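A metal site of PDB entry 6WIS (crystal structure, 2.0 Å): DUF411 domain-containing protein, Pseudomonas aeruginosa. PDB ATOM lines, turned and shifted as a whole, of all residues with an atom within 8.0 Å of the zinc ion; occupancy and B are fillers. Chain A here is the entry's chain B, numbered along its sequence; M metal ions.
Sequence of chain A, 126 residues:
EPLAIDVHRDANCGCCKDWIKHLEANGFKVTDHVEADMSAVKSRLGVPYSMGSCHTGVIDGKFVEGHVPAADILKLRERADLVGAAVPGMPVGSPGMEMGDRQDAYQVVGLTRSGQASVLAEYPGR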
ATOM      1  N   ASP A   6      35.393  -7.494  22.882  1.00  0.00           N
ATOM      2  CA  ASP A   6      34.590  -6.290  23.087  1.00  0.00           C
ATOM      3  C   ASP A   6      33.295  -6.689  23.793  1.00  0.00           C
ATOM      4  O   ASP A   6      32.676  -7.647  23.355  1.00  0.00           O
ATOM      5  CB  ASP A   6      34.485  -5.705  21.713  1.00  0.00           C
ATOM      6  CG  ASP A   6      33.725  -4.436  21.768  1.00  0.00           C
ATOM      7  OD1 ASP A   6      34.064  -3.569  22.556  1.00  0.00           O
ATOM      8  OD2 ASP A   6      32.763  -4.333  21.062  1.00  0.00           O
ATOM      9  N   VAL A   7      32.874  -5.938  24.819  1.00  0.00           N
ATOM     10  CA  VAL A   7      31.777  -6.368  25.694  1.00  0.00           C
ATOM     11  C   VAL A   7      30.710  -5.274  25.801  1.00  0.00           C
ATOM     12  O   VAL A   7      31.034  -4.114  26.127  1.00  0.00           O
ATOM     13  CB  VAL A   7      32.278  -6.763  27.099  1.00  0.00           C
ATOM     14  CG1 VAL A   7      31.069  -7.230  27.998  1.00  0.00           C
ATOM     15  CG2 VAL A   7      33.292  -7.851  27.004  1.00  0.00           C
ATOM     16  N   HIS A   8      29.459  -5.647  25.566  1.00  0.00           N
ATOM     17  CA  HIS A   8      28.310  -4.774  25.755  1.00  0.00           C
ATOM     18  C   HIS A   8      27.572  -5.285  26.974  1.00  0.00           C
ATOM     19  O   HIS A   8      27.126  -6.438  26.988  1.00  0.00           O
ATOM     20  CB  HIS A   8      27.361  -4.780  24.553  1.00  0.00           C
ATOM     21  CG  HIS A   8      28.035  -4.627  23.239  1.00  0.00           C
ATOM     22  ND1 HIS A   8      28.096  -3.436  22.557  1.00  0.00           N
ATOM     23  CD2 HIS A   8      28.659  -5.545  22.452  1.00  0.00           C
ATOM     24  CE1 HIS A   8      28.733  -3.612  21.418  1.00  0.00           C
ATOM     25  NE2 HIS A   8      29.088  -4.880  21.330  1.00  0.00           N
ATOM     26  N   ARG A   9      27.450  -4.456  28.008  1.00  0.00           N
ATOM     27  CA  ARG A   9      26.914  -4.977  29.249  1.00  0.00           C
ATOM     28  C   ARG A   9      25.763  -4.124  29.741  1.00  0.00           C
ATOM     29  O   ARG A   9      25.695  -2.917  29.478  1.00  0.00           O
ATOM     30  CB  ARG A   9      27.993  -5.109  30.350  1.00  0.00           C
ATOM     31  CG  ARG A   9      28.867  -3.876  30.595  1.00  0.00           C
ATOM     32  CD  ARG A   9      29.781  -4.051  31.810  1.00  0.00           C
ATOM     33  NE  ARG A   9      30.645  -2.883  31.964  1.00  0.00           N
ATOM     34  CZ  ARG A   9      30.429  -1.904  32.839  1.00  0.00           C
ATOM     35  NH1 ARG A   9      29.384  -1.937  33.666  1.00  0.00           N
ATOM     36  NH2 ARG A   9      31.272  -0.882  32.875  1.00  0.00           N
ATOM     37  N   ASP A  32      34.911  -2.360  26.980  1.00  0.00           N
ATOM     38  CA  ASP A  32      33.514  -2.551  27.333  1.00  0.00           C
ATOM     39  C   ASP A  32      32.791  -1.233  27.533  1.00  0.00           C
ATOM     40  O   ASP A  32      33.384  -0.227  27.923  1.00  0.00           O
ATOM     41  CB  ASP A  32      33.360  -3.391  28.613  1.00  0.00           C
ATOM     42  CG  ASP A  32      33.855  -2.656  29.822  1.00  0.00           C
ATOM     43  OD1 ASP A  32      35.071  -2.394  29.878  1.00  0.00           O
ATOM     44  OD2 ASP A  32      33.038  -2.283  30.680  1.00  0.00           O
ATOM     45  N   HIS A  33      31.494  -1.264  27.307  1.00  0.00           N
ATOM     46  CA  HIS A  33      30.667  -0.115  27.613  1.00  0.00           C
ATOM     47  C   HIS A  33      29.329  -0.596  28.148  1.00  0.00           C
ATOM     48  O   HIS A  33      28.884  -1.705  27.836  1.00  0.00           O
ATOM     49  CB  HIS A  33      30.444   0.767  26.396  1.00  0.00           C
ATOM     50  CG  HIS A  33      29.856   0.027  25.246  1.00  0.00           C
ATOM     51  ND1 HIS A  33      30.633  -0.588  24.284  1.00  0.00           N
ATOM     52  CD2 HIS A  33      28.566  -0.203  24.899  1.00  0.00           C
ATOM     53  CE1 HIS A  33      29.841  -1.158  23.391  1.00  0.00           C
ATOM     54  NE2 HIS A  33      28.591  -0.922  23.734  1.00  0.00           N
ATOM     55  N   VAL A  34      28.728   0.249  28.983  1.00  0.00           N
ATOM     56  CA  VAL A  34      27.342   0.049  29.374  1.00  0.00           C
ATOM     57  C   VAL A  34      26.471   0.243  28.140  1.00  0.00           C
ATOM     58  O   VAL A  34      26.735   1.141  27.304  1.00  0.00           O
ATOM     59  CB  VAL A  34      26.951   0.990  30.526  1.00  0.00           C
ATOM     60  CG1 VAL A  34      25.454   1.117  30.657  1.00  0.00           C
ATOM     61  CG2 VAL A  34      27.547   0.489  31.861  1.00  0.00           C
ATOM     62  N   GLU A  35      25.446  -0.586  28.003  1.00  0.00           N
ATOM     63  CA  GLU A  35      24.697  -0.734  26.766  1.00  0.00           C
ATOM     64  C   GLU A  35      23.428   0.099  26.788  1.00  0.00           C
ATOM     65  O   GLU A  35      22.647   0.004  27.743  1.00  0.00           O
ATOM     66  CB  GLU A  35      24.292  -2.192  26.552  1.00  0.00           C
ATOM     67  CG  GLU A  35      23.306  -2.305  25.415  1.00  0.00           C
ATOM     68  CD  GLU A  35      23.990  -1.862  24.193  1.00  0.00           C
ATOM     69  OE1 GLU A  35      25.163  -2.171  24.177  1.00  0.00           O
ATOM     70  OE2 GLU A  35      23.456  -1.191  23.298  1.00  0.00           O
ATOM     71  N   ALA A  36      23.164   0.846  25.719  1.00  0.00           N
ATOM     72  CA  ALA A  36      21.901   1.592  25.633  1.00  0.00           C
ATOM     73  C   ALA A  36      20.800   0.848  24.888  1.00  0.00           C
ATOM     74  O   ALA A  36      19.618   1.043  25.183  1.00  0.00           O
ATOM     75  CB  ALA A  36      22.127   2.954  24.977  1.00  0.00           C
ATOM     76  N   ASP A  37      21.145   0.003  23.913  1.00  0.00           N
ATOM     77  CA  ASP A  37      20.154  -0.684  23.071  1.00  0.00           C
ATOM     78  C   ASP A  37      20.542  -2.162  22.966  1.00  0.00           C
ATOM     79  O   ASP A  37      20.945  -2.628  21.896  1.00  0.00           O
ATOM     80  CB  ASP A  37      20.062  -0.010  21.691  1.00  0.00           C
ATOM     81  CG  ASP A  37      19.246   1.277  21.718  1.00  0.00           C
ATOM     82  OD1 ASP A  37      18.180   1.295  22.377  1.00  0.00           O
ATOM     83  OD2 ASP A  37      19.677   2.267  21.094  1.00  0.00           O
ATOM     84  N   MET A  38      20.409  -2.889  24.070  1.00  0.00           N
ATOM     85  CA  MET A  38      20.851  -4.290  24.129  1.00  0.00           C
ATOM     86  C   MET A  38      20.084  -5.224  23.198  1.00  0.00           C
ATOM     87  O   MET A  38      20.652  -6.176  22.643  1.00  0.00           O
ATOM     88  CB  MET A  38      20.728  -4.833  25.556  1.00  0.00           C
ATOM     89  CG  MET A  38      21.316  -6.238  25.688  1.00  0.00           C
ATOM     90  SD  MET A  38      23.248  -6.312  25.318  1.00  0.00           S
ATOM     91  CE  MET A  38      23.877  -5.592  27.018  1.00  0.00           C
ATOM     92  N   VAL A  41      21.516  -4.983  19.926  1.00  0.00           N
ATOM     93  CA  VAL A  41      22.830  -5.640  19.884  1.00  0.00           C
ATOM     94  C   VAL A  41      22.672  -7.143  19.704  1.00  0.00           C
ATOM     95  O   VAL A  41      23.325  -7.760  18.863  1.00  0.00           O
ATOM     96  CB  VAL A  41      23.641  -5.307  21.148  1.00  0.00           C
ATOM     97  CG1 VAL A  41      24.759  -6.311  21.357  1.00  0.00           C
ATOM     98  CG2 VAL A  41      24.199  -3.887  21.065  1.00  0.00           C
ATOM     99  N   THR A  56      26.713  -9.170  26.346  1.00  0.00           N
ATOM    100  CA  THR A  56      27.062  -9.798  25.078  1.00  0.00           C
ATOM    101  C   THR A  56      28.445  -9.338  24.670  1.00  0.00           C
ATOM    102  O   THR A  56      28.680  -8.141  24.499  1.00  0.00           O
ATOM    103  CB  THR A  56      26.049  -9.448  23.971  1.00  0.00           C
ATOM    104  OG1 THR A  56      24.725  -9.865  24.367  1.00  0.00           O
ATOM    105  CG2 THR A  56      26.446 -10.156  22.654  1.00  0.00           C
HETATM  106 ZN    ZN M   1      26.918  -1.692  22.791  1.00  0.00          ZN
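The backbone carbonyl oxygen of Thr 56 lies within hydrogen-bond range of the backbone NH of His 8. O of His 33 is in hydrogen-bond range of N of Arg 9 (3.1 Å). N of His 33 is in hydrogen-bond range of O of Val 7, at 3.1 Å. The backbone NH (N) of Glu 35 is in hydrogen-bond range of the backbone carbonyl oxygen (O) of Arg 9. The side-chain carboxylate (OE2) of Glu 35 sits at hydrogen-bond distance from the backbone NH (N) of Asp 37 (2.7 Å).
The zinc ion is bound by NE2 of His 33. ND1 of His 8 is bound to the zinc ion (2.1 Å). The zinc ion is bound by the side-chain carboxylate (OE1) of Glu 35, 2.3 Å away.
Residues that only touch the zinc ion: Val 41. Four residues have an atom within 4 Å of the zinc ion: His 8, His 33, Glu 35 and Val 41. The nearest printed residue that does not touch the zinc ion is Val 34 (5.3 Å).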
